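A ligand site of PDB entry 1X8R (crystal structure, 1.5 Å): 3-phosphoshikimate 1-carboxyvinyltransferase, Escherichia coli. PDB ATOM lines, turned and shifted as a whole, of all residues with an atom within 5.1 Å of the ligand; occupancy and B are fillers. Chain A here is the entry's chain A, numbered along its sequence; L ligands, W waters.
An oxygen (O10) of the ligand is in hydrogen-bond range of a ring nitrogen (NE2) of His 385 (2.9 Å).
An oxygen (O10) of the ligand is in salt-bridge range of the guanidinium group (NH1) of Arg 344 (3.1 Å).
NH1 of Arg 124 is in salt-bridge range of O13 of the ligand (2.7 Å).
The side-chain hydroxyl (OG) of Ser 23 is in hydrogen-bond range of an oxygen (O5) of the ligand (2.7 Å).
O8 of the ligand sits at hydrogen-bond distance from OG of Ser 169, 2.7 Å away.
The side-chain amide nitrogen (NE2) of Gln 171 is in hydrogen-bond range of an oxygen (O13) of the ligand (2.8 Å).
The guanidinium group (NH1) of Arg 27 is in salt-bridge range of an oxygen (O4) of the ligand (2.7 Å).
OE2 of Glu 341 lies close to O11 of the ligand (2.6 Å).
The side-chain amino group (NZ) of Lys 411 is in salt-bridge range of an oxygen (O11) of the ligand, 2.6 Å away.
OG of Ser 170 sits at hydrogen-bond distance from O6 of the ligand, at 2.5 Å.
The side-chain carboxylate (OD1) of Asp 313 sits at hydrogen-bond distance from an oxygen (O2) of the ligand, 3.0 Å away.
The side-chain hydroxyl (OG) of Ser 197 is in hydrogen-bond range of an oxygen (O7) of the ligand (2.6 Å).
An oxygen (O7) of the ligand is in salt-bridge range of the side-chain amino group of Lys 340, 2.7 Å away.
NZ of Lys 22 lies within salt-bridge range of O9 of the ligand, 2.6 Å away.
The guanidinium group of Arg 386 is in salt-bridge range of an oxygen (O9) of the ligand.
An oxygen (O6) of the ligand is in hydrogen-bond range of the backbone NH (N) of Ser 170 (2.7 Å).
The side-chain amide nitrogen (ND2) of Asn 336 sits at hydrogen-bond distance from an oxygen (O7) of the ligand, 2.9 Å away.
The side-chain amide oxygen of Gln 171 sits at hydrogen-bond distance from the guanidinium group of Arg 100, 2.8 Å away.
The side-chain carboxylate (OD2) of Asp 313 is in salt-bridge range of the guanidinium group (NH2) of Arg 344, at 3.0 Å.
The side-chain amino group of Lys 411 lies within salt-bridge range of the side-chain carboxylate of Asp 49, at 2.9 Å.
The side-chain amino group (NZ) of Lys 340 is in salt-bridge range of the side-chain carboxylate (OD2) of Asp 313, at 3.9 Å.
The guanidinium group (NH1) of Arg 27 lies within hydrogen-bond range of the backbone carbonyl oxygen (O) of Tyr 200 (3.3 Å).
The side-chain amino group (NZ) of Lys 411 lies within salt-bridge range of the side-chain carboxylate (OE2) of Glu 341 (3.0 Å).
The side-chain hydroxyl (OG) of Ser 169 is in hydrogen-bond range of the backbone NH (N) of Gln 171.
OG1 of Thr 412 lies within hydrogen-bond range of ND1 of His 385 (2.8 Å).
Water W4 lies within hydrogen-bond range of O12 of the ligand, OG1 of Thr 97, OD2 of Asp 49 and N of Gly 96.
Water W1 lies within hydrogen-bond range of an oxygen (O8) of the ligand (2.6 Å), the backbone carbonyl oxygen (O) of Val 168 (3.0 Å) and the side-chain amide nitrogen (ND2) of Asn 336 (3.5 Å).
Water W2 lies within hydrogen-bond range of OG1 of Thr 174, OG of Ser 170, O4 of the ligand, NH1 of Arg 27 and N of Gln 171.
O of Asn 94 touches O11 of the ligand, at 3.6 Å.
N of Gly 96 touches O11 of the ligand (3.5 Å).
Thr 97 touches the ligand (CG2 to O5, 3.4 Å).
Tyr 200 touches the ligand (CD2 to C2, 3.4 Å).
Of the 28 residues printed, 20 come within 4 Å of the ligand.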
ATOM      1  N   LYS A  22      -8.476  24.612 -26.932  1.00  0.00           N
ATOM      2  CA  LYS A  22      -7.749  24.635 -25.663  1.00  0.00           C
ATOM      3  C   LYS A  22      -7.746  23.251 -25.021  1.00  0.00           C
ATOM      4  O   LYS A  22      -6.710  22.816 -24.509  1.00  0.00           O
ATOM      5  CB  LYS A  22      -8.398  25.646 -24.701  1.00  0.00           C
ATOM      6  CG  LYS A  22      -7.814  25.631 -23.275  1.00  0.00           C
ATOM      7  CD  LYS A  22      -8.770  24.903 -22.308  1.00  0.00           C
ATOM      8  CE  LYS A  22      -9.996  25.776 -21.982  1.00  0.00           C
ATOM      9  NZ  LYS A  22     -11.102  25.064 -21.264  1.00  0.00           N
ATOM     10  N   SER A  23      -8.889  22.547 -25.069  1.00  0.00           N
ATOM     11  CA  SER A  23      -8.996  21.216 -24.481  1.00  0.00           C
ATOM     12  C   SER A  23      -8.027  20.244 -25.105  1.00  0.00           C
ATOM     13  O   SER A  23      -7.378  19.452 -24.410  1.00  0.00           O
ATOM     14  CB  SER A  23     -10.426  20.681 -24.668  1.00  0.00           C
ATOM     15  OG  SER A  23     -11.338  21.419 -23.863  1.00  0.00           O
ATOM     16  N   ARG A  27      -4.101  18.867 -23.483  1.00  0.00           N
ATOM     17  CA  ARG A  27      -3.954  17.420 -23.364  1.00  0.00           C
ATOM     18  C   ARG A  27      -2.766  16.966 -24.222  1.00  0.00           C
ATOM     19  O   ARG A  27      -1.953  16.158 -23.760  1.00  0.00           O
ATOM     20  CB  ARG A  27      -5.204  16.700 -23.848  1.00  0.00           C
ATOM     21  CG  ARG A  27      -6.348  16.677 -22.819  1.00  0.00           C
ATOM     22  CD  ARG A  27      -7.615  16.245 -23.545  1.00  0.00           C
ATOM     23  NE  ARG A  27      -8.780  16.042 -22.709  1.00  0.00           N
ATOM     24  CZ  ARG A  27      -9.540  17.014 -22.210  1.00  0.00           C
ATOM     25  NH1 ARG A  27     -10.611  16.719 -21.476  1.00  0.00           N
ATOM     26  NH2 ARG A  27      -9.228  18.292 -22.438  1.00  0.00           N
ATOM     27  N   ASP A  49      -4.149  29.835 -20.977  1.00  0.00           N
ATOM     28  CA  ASP A  49      -4.160  28.473 -20.454  1.00  0.00           C
ATOM     29  C   ASP A  49      -3.057  27.621 -21.040  1.00  0.00           C
ATOM     30  O   ASP A  49      -2.480  26.805 -20.327  1.00  0.00           O
ATOM     31  CB  ASP A  49      -5.491  27.774 -20.731  1.00  0.00           C
ATOM     32  CG  ASP A  49      -6.589  28.168 -19.767  1.00  0.00           C
ATOM     33  OD1 ASP A  49      -6.391  28.972 -18.839  1.00  0.00           O
ATOM     34  OD2 ASP A  49      -7.714  27.618 -19.952  1.00  0.00           O
ATOM     35  N   ASN A  94      -5.485  30.209 -14.394  1.00  0.00           N
ATOM     36  CA  ASN A  94      -6.857  29.791 -14.174  1.00  0.00           C
ATOM     37  C   ASN A  94      -7.128  28.564 -15.025  1.00  0.00           C
ATOM     38  O   ASN A  94      -8.286  28.265 -15.308  1.00  0.00           O
ATOM     39  CB  ASN A  94      -7.827  30.890 -14.613  1.00  0.00           C
ATOM     40  CG  ASN A  94      -7.574  32.221 -13.922  1.00  0.00           C
ATOM     41  OD1 ASN A  94      -7.837  32.378 -12.734  1.00  0.00           O
ATOM     42  ND2 ASN A  94      -7.042  33.187 -14.676  1.00  0.00           N
ATOM     43  N   ALA A  95      -6.080  27.835 -15.400  1.00  0.00           N
ATOM     44  CA  ALA A  95      -6.236  26.688 -16.282  1.00  0.00           C
ATOM     45  C   ALA A  95      -6.611  25.364 -15.644  1.00  0.00           C
ATOM     46  O   ALA A  95      -5.762  24.670 -15.100  1.00  0.00           O
ATOM     47  CB  ALA A  95      -4.959  26.503 -17.084  1.00  0.00           C
ATOM     48  N   GLY A  96      -7.885  24.999 -15.753  1.00  0.00           N
ATOM     49  CA  GLY A  96      -8.314  23.739 -15.177  1.00  0.00           C
ATOM     50  C   GLY A  96      -7.643  22.581 -15.894  1.00  0.00           C
ATOM     51  O   GLY A  96      -7.291  21.580 -15.257  1.00  0.00           O
ATOM     52  N   THR A  97      -7.432  22.731 -17.206  1.00  0.00           N
ATOM     53  CA  THR A  97      -6.824  21.677 -17.997  1.00  0.00           C
ATOM     54  C   THR A  97      -5.334  21.551 -17.744  1.00  0.00           C
ATOM     55  O   THR A  97      -4.683  20.699 -18.338  1.00  0.00           O
ATOM     56  CB  THR A  97      -7.088  21.864 -19.499  1.00  0.00           C
ATOM     57  OG1 THR A  97      -6.572  23.128 -19.923  1.00  0.00           O
ATOM     58  CG2 THR A  97      -8.574  21.832 -19.777  1.00  0.00           C
ATOM     59  N   ARG A 100      -5.848  20.214 -13.127  1.00  0.00           N
ATOM     60  CA  ARG A 100      -6.323  18.865 -12.839  1.00  0.00           C
ATOM     61  C   ARG A 100      -5.398  17.781 -13.437  1.00  0.00           C
ATOM     62  O   ARG A 100      -4.969  16.880 -12.724  1.00  0.00           O
ATOM     63  CB  ARG A 100      -7.775  18.688 -13.318  1.00  0.00           C
ATOM     64  CG  ARG A 100      -8.833  19.214 -12.315  1.00  0.00           C
ATOM     65  CD  ARG A 100      -8.794  20.769 -12.145  1.00  0.00           C
ATOM     66  NE  ARG A 100      -9.886  21.256 -11.295  1.00  0.00           N
ATOM     67  CZ  ARG A 100     -11.104  21.575 -11.738  1.00  0.00           C
ATOM     68  NH1 ARG A 100     -12.018  22.021 -10.887  1.00  0.00           N
ATOM     69  NH2 ARG A 100     -11.403  21.469 -13.024  1.00  0.00           N
ATOM     70  N   ARG A 124     -11.690  26.641  -6.962  1.00  0.00           N
ATOM     71  CA  ARG A 124     -12.261  25.635  -7.870  1.00  0.00           C
ATOM     72  C   ARG A 124     -11.907  24.300  -7.253  1.00  0.00           C
ATOM     73  O   ARG A 124     -10.746  23.990  -6.987  1.00  0.00           O
ATOM     74  CB  ARG A 124     -11.696  25.779  -9.280  1.00  0.00           C
ATOM     75  CG  ARG A 124     -12.157  27.097  -9.917  1.00  0.00           C
ATOM     76  CD  ARG A 124     -11.776  27.235 -11.383  1.00  0.00           C
ATOM     77  NE  ARG A 124     -12.332  26.145 -12.181  1.00  0.00           N
ATOM     78  CZ  ARG A 124     -12.013  25.911 -13.451  1.00  0.00           C
ATOM     79  NH1 ARG A 124     -12.560  24.888 -14.098  1.00  0.00           N
ATOM     80  NH2 ARG A 124     -11.161  26.721 -14.078  1.00  0.00           N
ATOM     81  N   VAL A 168     -19.099  16.361 -10.274  1.00  0.00           N
ATOM     82  CA  VAL A 168     -18.778  17.781 -10.286  1.00  0.00           C
ATOM     83  C   VAL A 168     -17.944  18.211 -11.490  1.00  0.00           C
ATOM     84  O   VAL A 168     -18.196  19.272 -12.070  1.00  0.00           O
ATOM     85  CB  VAL A 168     -18.053  18.176  -8.990  1.00  0.00           C
ATOM     86  CG1 VAL A 168     -17.565  19.615  -9.085  1.00  0.00           C
ATOM     87  CG2 VAL A 168     -18.989  18.058  -7.816  1.00  0.00           C
ATOM     88  N   SER A 169     -16.938  17.427 -11.852  1.00  0.00           N
ATOM     89  CA  SER A 169     -16.127  17.756 -13.010  1.00  0.00           C
ATOM     90  C   SER A 169     -15.661  16.502 -13.718  1.00  0.00           C
ATOM     91  O   SER A 169     -15.325  15.513 -13.071  1.00  0.00           O
ATOM     92  CB  SER A 169     -14.878  18.564 -12.618  1.00  0.00           C
ATOM     93  OG  SER A 169     -14.070  18.754 -13.764  1.00  0.00           O
ATOM     94  N   SER A 170     -15.657  16.533 -15.050  1.00  0.00           N
ATOM     95  CA  SER A 170     -15.142  15.401 -15.785  1.00  0.00           C
ATOM     96  C   SER A 170     -13.625  15.440 -15.755  1.00  0.00           C
ATOM     97  O   SER A 170     -12.977  14.438 -16.044  1.00  0.00           O
ATOM     98  CB  SER A 170     -15.594  15.460 -17.253  1.00  0.00           C
ATOM     99  OG  SER A 170     -15.006  16.573 -17.941  1.00  0.00           O
ATOM    100  N   GLN A 171     -13.053  16.590 -15.403  1.00  0.00           N
ATOM    101  CA  GLN A 171     -11.604  16.704 -15.411  1.00  0.00           C
ATOM    102  C   GLN A 171     -10.876  15.803 -14.430  1.00  0.00           C
ATOM    103  O   GLN A 171      -9.704  15.484 -14.631  1.00  0.00           O
ATOM    104  CB  GLN A 171     -11.206  18.156 -15.177  1.00  0.00           C
ATOM    105  CG  GLN A 171     -11.690  19.083 -16.275  1.00  0.00           C
ATOM    106  CD  GLN A 171     -11.026  20.448 -16.205  1.00  0.00           C
ATOM    107  OE1 GLN A 171     -10.131  20.683 -15.410  1.00  0.00           O
ATOM    108  NE2 GLN A 171     -11.457  21.349 -17.083  1.00  0.00           N
ATOM    109  N   THR A 174     -10.616  12.616 -16.290  1.00  0.00           N
ATOM    110  CA  THR A 174      -9.652  12.844 -17.359  1.00  0.00           C
ATOM    111  C   THR A 174      -8.216  12.750 -16.839  1.00  0.00           C
ATOM    112  O   THR A 174      -7.359  12.099 -17.441  1.00  0.00           O
ATOM    113  CB  THR A 174      -9.888  14.234 -17.994  1.00  0.00           C
ATOM    114  OG1 THR A 174     -10.942  14.111 -18.949  1.00  0.00           O
ATOM    115  CG2 THR A 174      -8.637  14.776 -18.659  1.00  0.00           C
ATOM    116  N   VAL A 196     -20.676  13.968 -15.178  1.00  0.00           N
ATOM    117  CA  VAL A 196     -21.059  15.157 -15.922  1.00  0.00           C
ATOM    118  C   VAL A 196     -20.023  15.446 -17.002  1.00  0.00           C
ATOM    119  O   VAL A 196     -18.907  14.895 -16.991  1.00  0.00           O
ATOM    120  CB  VAL A 196     -21.160  16.411 -15.006  1.00  0.00           C
ATOM    121  CG1 VAL A 196     -22.269  16.235 -13.985  1.00  0.00           C
ATOM    122  CG2 VAL A 196     -19.810  16.668 -14.324  1.00  0.00           C
ATOM    123  N   SER A 197     -20.422  16.296 -17.949  1.00  0.00           N
ATOM    124  CA  SER A 197     -19.530  16.697 -19.055  1.00  0.00           C
ATOM    125  C   SER A 197     -18.869  15.500 -19.735  1.00  0.00           C
ATOM    126  O   SER A 197     -17.699  15.537 -20.102  1.00  0.00           O
ATOM    127  CB  SER A 197     -18.449  17.658 -18.534  1.00  0.00           C
ATOM    128  OG  SER A 197     -19.050  18.819 -17.964  1.00  0.00           O
ATOM    129  N   TYR A 200     -16.151  15.329 -22.715  1.00  0.00           N
ATOM    130  CA  TYR A 200     -14.748  15.645 -22.505  1.00  0.00           C
ATOM    131  C   TYR A 200     -13.917  14.408 -22.211  1.00  0.00           C
ATOM    132  O   TYR A 200     -12.705  14.392 -22.478  1.00  0.00           O
ATOM    133  CB  TYR A 200     -14.576  16.706 -21.398  1.00  0.00           C
ATOM    134  CG  TYR A 200     -15.080  18.055 -21.849  1.00  0.00           C
ATOM    135  CD1 TYR A 200     -16.379  18.460 -21.576  1.00  0.00           C
ATOM    136  CD2 TYR A 200     -14.242  18.927 -22.551  1.00  0.00           C
ATOM    137  CE1 TYR A 200     -16.846  19.707 -21.970  1.00  0.00           C
ATOM    138  CE2 TYR A 200     -14.697  20.178 -22.940  1.00  0.00           C
ATOM    139  CZ  TYR A 200     -15.999  20.575 -22.652  1.00  0.00           C
ATOM    140  OH  TYR A 200     -16.439  21.846 -22.978  1.00  0.00           O
ATOM    141  N   PRO A 312     -21.773  22.048 -21.439  1.00  0.00           N
ATOM    142  CA  PRO A 312     -21.831  23.092 -20.425  1.00  0.00           C
ATOM    143  C   PRO A 312     -21.290  24.478 -20.765  1.00  0.00           C
ATOM    144  O   PRO A 312     -21.926  25.454 -20.407  1.00  0.00           O
ATOM    145  CB  PRO A 312     -21.119  22.467 -19.229  1.00  0.00           C
ATOM    146  CG  PRO A 312     -20.108  21.563 -19.859  1.00  0.00           C
ATOM    147  CD  PRO A 312     -20.904  20.940 -21.005  1.00  0.00           C
ATOM    148  N   ASP A 313     -20.169  24.541 -21.475  1.00  0.00           N
ATOM    149  CA  ASP A 313     -19.572  25.843 -21.818  1.00  0.00           C
ATOM    150  C   ASP A 313     -20.304  26.520 -22.975  1.00  0.00           C
ATOM    151  O   ASP A 313     -20.659  27.712 -22.886  1.00  0.00           O
ATOM    152  CB  ASP A 313     -18.105  25.665 -22.221  1.00  0.00           C
ATOM    153  CG  ASP A 313     -17.183  25.499 -21.036  1.00  0.00           C
ATOM    154  OD1 ASP A 313     -16.008  25.129 -21.274  1.00  0.00           O
ATOM    155  OD2 ASP A 313     -17.589  25.732 -19.881  1.00  0.00           O
ATOM    156  N   ASN A 336     -22.598  22.599 -12.520  1.00  0.00           N
ATOM    157  CA  ASN A 336     -21.201  22.958 -12.409  1.00  0.00           C
ATOM    158  C   ASN A 336     -20.792  24.287 -13.016  1.00  0.00           C
ATOM    159  O   ASN A 336     -19.625  24.681 -12.948  1.00  0.00           O
ATOM    160  CB  ASN A 336     -20.281  21.765 -12.772  1.00  0.00           C
ATOM    161  CG  ASN A 336     -20.068  21.569 -14.261  1.00  0.00           C
ATOM    162  OD1 ASN A 336     -20.528  22.348 -15.100  1.00  0.00           O
ATOM    163  ND2 ASN A 336     -19.318  20.523 -14.581  1.00  0.00           N
ATOM    164  N   LYS A 340     -16.787  27.041 -11.739  1.00  0.00           N
ATOM    165  CA  LYS A 340     -15.761  27.319 -12.732  1.00  0.00           C
ATOM    166  C   LYS A 340     -15.092  28.690 -12.548  1.00  0.00           C
ATOM    167  O   LYS A 340     -14.864  29.091 -11.403  1.00  0.00           O
ATOM    168  CB  LYS A 340     -16.371  27.083 -14.108  1.00  0.00           C
ATOM    169  CG  LYS A 340     -16.536  25.592 -14.321  1.00  0.00           C
ATOM    170  CD  LYS A 340     -17.349  25.224 -15.532  1.00  0.00           C
ATOM    171  CE  LYS A 340     -17.322  23.700 -15.690  1.00  0.00           C
ATOM    172  NZ  LYS A 340     -18.038  23.235 -16.911  1.00  0.00           N
ATOM    173  N   GLU A 341     -14.761  29.413 -13.625  1.00  0.00           N
ATOM    174  CA  GLU A 341     -14.085  30.716 -13.494  1.00  0.00           C
ATOM    175  C   GLU A 341     -14.782  31.651 -12.526  1.00  0.00           C
ATOM    176  O   GLU A 341     -14.152  32.490 -11.895  1.00  0.00           O
ATOM    177  CB  GLU A 341     -13.930  31.384 -14.853  1.00  0.00           C
ATOM    178  CG  GLU A 341     -12.812  30.797 -15.716  1.00  0.00           C
ATOM    179  CD  GLU A 341     -12.917  29.292 -15.925  1.00  0.00           C
ATOM    180  OE1 GLU A 341     -14.043  28.765 -15.995  1.00  0.00           O
ATOM    181  OE2 GLU A 341     -11.860  28.639 -16.028  1.00  0.00           O
ATOM    182  N   ARG A 344     -21.062  30.810 -12.632  1.00  0.00           N
ATOM    183  CA  ARG A 344     -21.685  31.293 -13.858  1.00  0.00           C
ATOM    184  C   ARG A 344     -23.201  31.387 -13.836  1.00  0.00           C
ATOM    185  O   ARG A 344     -23.761  32.128 -14.617  1.00  0.00           O
ATOM    186  CB  ARG A 344     -21.231  30.458 -15.044  1.00  0.00           C
ATOM    187  CG  ARG A 344     -19.738  30.651 -15.352  1.00  0.00           C
ATOM    188  CD  ARG A 344     -19.188  29.532 -16.236  1.00  0.00           C
ATOM    189  NE  ARG A 344     -17.939  29.959 -16.873  1.00  0.00           N
ATOM    190  CZ  ARG A 344     -17.147  29.173 -17.603  1.00  0.00           C
ATOM    191  NH1 ARG A 344     -16.039  29.673 -18.146  1.00  0.00           N
ATOM    192  NH2 ARG A 344     -17.440  27.885 -17.786  1.00  0.00           N
ATOM    193  N   HIS A 385     -13.503  34.509 -19.169  1.00  0.00           N
ATOM    194  CA  HIS A 385     -13.488  34.654 -20.622  1.00  0.00           C
ATOM    195  C   HIS A 385     -14.832  34.441 -21.283  1.00  0.00           C
ATOM    196  O   HIS A 385     -15.197  35.190 -22.202  1.00  0.00           O
ATOM    197  CB  HIS A 385     -12.445  33.672 -21.222  1.00  0.00           C
ATOM    198  CG  HIS A 385     -12.685  32.224 -20.922  1.00  0.00           C
ATOM    199  ND1 HIS A 385     -12.361  31.234 -21.826  1.00  0.00           N
ATOM    200  CD2 HIS A 385     -13.150  31.588 -19.816  1.00  0.00           C
ATOM    201  CE1 HIS A 385     -12.618  30.052 -21.283  1.00  0.00           C
ATOM    202  NE2 HIS A 385     -13.095  30.240 -20.075  1.00  0.00           N
ATOM    203  N   ARG A 386     -15.598  33.471 -20.793  1.00  0.00           N
ATOM    204  CA  ARG A 386     -16.880  33.220 -21.450  1.00  0.00           C
ATOM    205  C   ARG A 386     -17.954  34.244 -21.152  1.00  0.00           C
ATOM    206  O   ARG A 386     -18.853  34.426 -21.954  1.00  0.00           O
ATOM    207  CB  ARG A 386     -17.366  31.809 -21.140  1.00  0.00           C
ATOM    208  CG  ARG A 386     -16.376  30.774 -21.647  1.00  0.00           C
ATOM    209  CD  ARG A 386     -17.002  29.398 -21.852  1.00  0.00           C
ATOM    210  NE  ARG A 386     -15.903  28.468 -22.116  1.00  0.00           N
ATOM    211  CZ  ARG A 386     -15.171  28.437 -23.218  1.00  0.00           C
ATOM    212  NH1 ARG A 386     -14.174  27.552 -23.287  1.00  0.00           N
ATOM    213  NH2 ARG A 386     -15.436  29.206 -24.273  1.00  0.00           N
ATOM    214  N   LYS A 411      -7.881  33.935 -21.884  1.00  0.00           N
ATOM    215  CA  LYS A 411      -7.730  32.632 -21.277  1.00  0.00           C
ATOM    216  C   LYS A 411      -7.742  31.565 -22.373  1.00  0.00           C
ATOM    217  O   LYS A 411      -6.957  30.598 -22.332  1.00  0.00           O
ATOM    218  CB  LYS A 411      -8.875  32.357 -20.295  1.00  0.00           C
ATOM    219  CG  LYS A 411      -8.614  31.162 -19.396  1.00  0.00           C
ATOM    220  CD  LYS A 411      -9.723  30.974 -18.383  1.00  0.00           C
ATOM    221  CE  LYS A 411      -9.504  29.757 -17.499  1.00  0.00           C
ATOM    222  NZ  LYS A 411      -9.827  28.459 -18.186  1.00  0.00           N
ATOM    223  N   THR A 412      -8.643  31.747 -23.340  1.00  0.00           N
ATOM    224  CA  THR A 412      -8.775  30.836 -24.479  1.00  0.00           C
ATOM    225  C   THR A 412      -8.817  31.487 -25.836  1.00  0.00           C
ATOM    226  O   THR A 412      -8.705  30.800 -26.845  1.00  0.00           O
ATOM    227  CB  THR A 412     -10.061  29.983 -24.408  1.00  0.00           C
ATOM    228  OG1 THR A 412     -11.220  30.838 -24.372  1.00  0.00           O
ATOM    229  CG2 THR A 412     -10.036  29.057 -23.210  1.00  0.00           C
HETATM  230  C1  LIG L   1     -12.774  20.760 -19.965  1.00  0.00           C
HETATM  231  C2  LIG L   1     -14.003  20.214 -19.461  1.00  0.00           C
HETATM  232  C3  LIG L   1     -15.079  21.151 -18.936  1.00  0.00           C
HETATM  233  C4  LIG L   1     -14.928  22.671 -19.485  1.00  0.00           C
HETATM  234  C5  LIG L   1     -13.498  23.160 -19.127  1.00  0.00           C
HETATM  235  C6  LIG L   1     -12.507  22.261 -19.997  1.00  0.00           C
HETATM  236  C7  LIG L   1     -11.729  19.842 -20.493  1.00  0.00           C
HETATM  237  O1  LIG L   1     -15.080  21.069 -17.341  1.00  0.00           O
HETATM  238  O2  LIG L   1     -15.981  23.389 -18.845  1.00  0.00           O
HETATM  239  O3  LIG L   1     -13.327  24.526 -19.517  1.00  0.00           O
HETATM  240  O4  LIG L   1     -11.604  18.740 -19.958  1.00  0.00           O
HETATM  241  O5  LIG L   1     -11.083  20.249 -21.410  1.00  0.00           O
HETATM  242  P1  LIG L   1     -16.103  20.121 -16.389  1.00  0.00           P
HETATM  243  O6  LIG L   1     -15.757  18.665 -16.724  1.00  0.00           O
HETATM  244  O7  LIG L   1     -17.551  20.561 -16.837  1.00  0.00           O
HETATM  245  O8  LIG L   1     -15.621  20.548 -14.989  1.00  0.00           O
HETATM  246  C8  LIG L   1     -13.074  25.589 -18.487  1.00  0.00           C
HETATM  247  C9  LIG L   1     -14.028  25.622 -17.194  1.00  0.00           C
HETATM  248  C10 LIG L   1     -12.999  26.941 -19.207  1.00  0.00           C
HETATM  249  O9  LIG L   1     -12.468  27.033 -20.361  1.00  0.00           O
HETATM  250  O10 LIG L   1     -13.628  27.851 -18.600  1.00  0.00           O
HETATM  251  P2  LIG L   1     -11.430  25.128 -17.648  1.00  0.00           P
HETATM  252  O11 LIG L   1     -10.898  26.424 -16.972  1.00  0.00           O
HETATM  253  O12 LIG L   1     -10.463  24.702 -18.714  1.00  0.00           O
HETATM  254  O13 LIG L   1     -11.693  24.044 -16.551  1.00  0.00           O
HETATM  255  O   HOH W   1     -16.549  21.636 -12.774  1.00  0.00           O
HETATM  256  O   HOH W   2     -12.384  16.395 -18.702  1.00  0.00           O
HETATM  257  O   HOH W   3     -13.727  22.324 -14.732  1.00  0.00           O
HETATM  258  O   HOH W   4      -7.971  25.166 -18.871  1.00  0.00           O
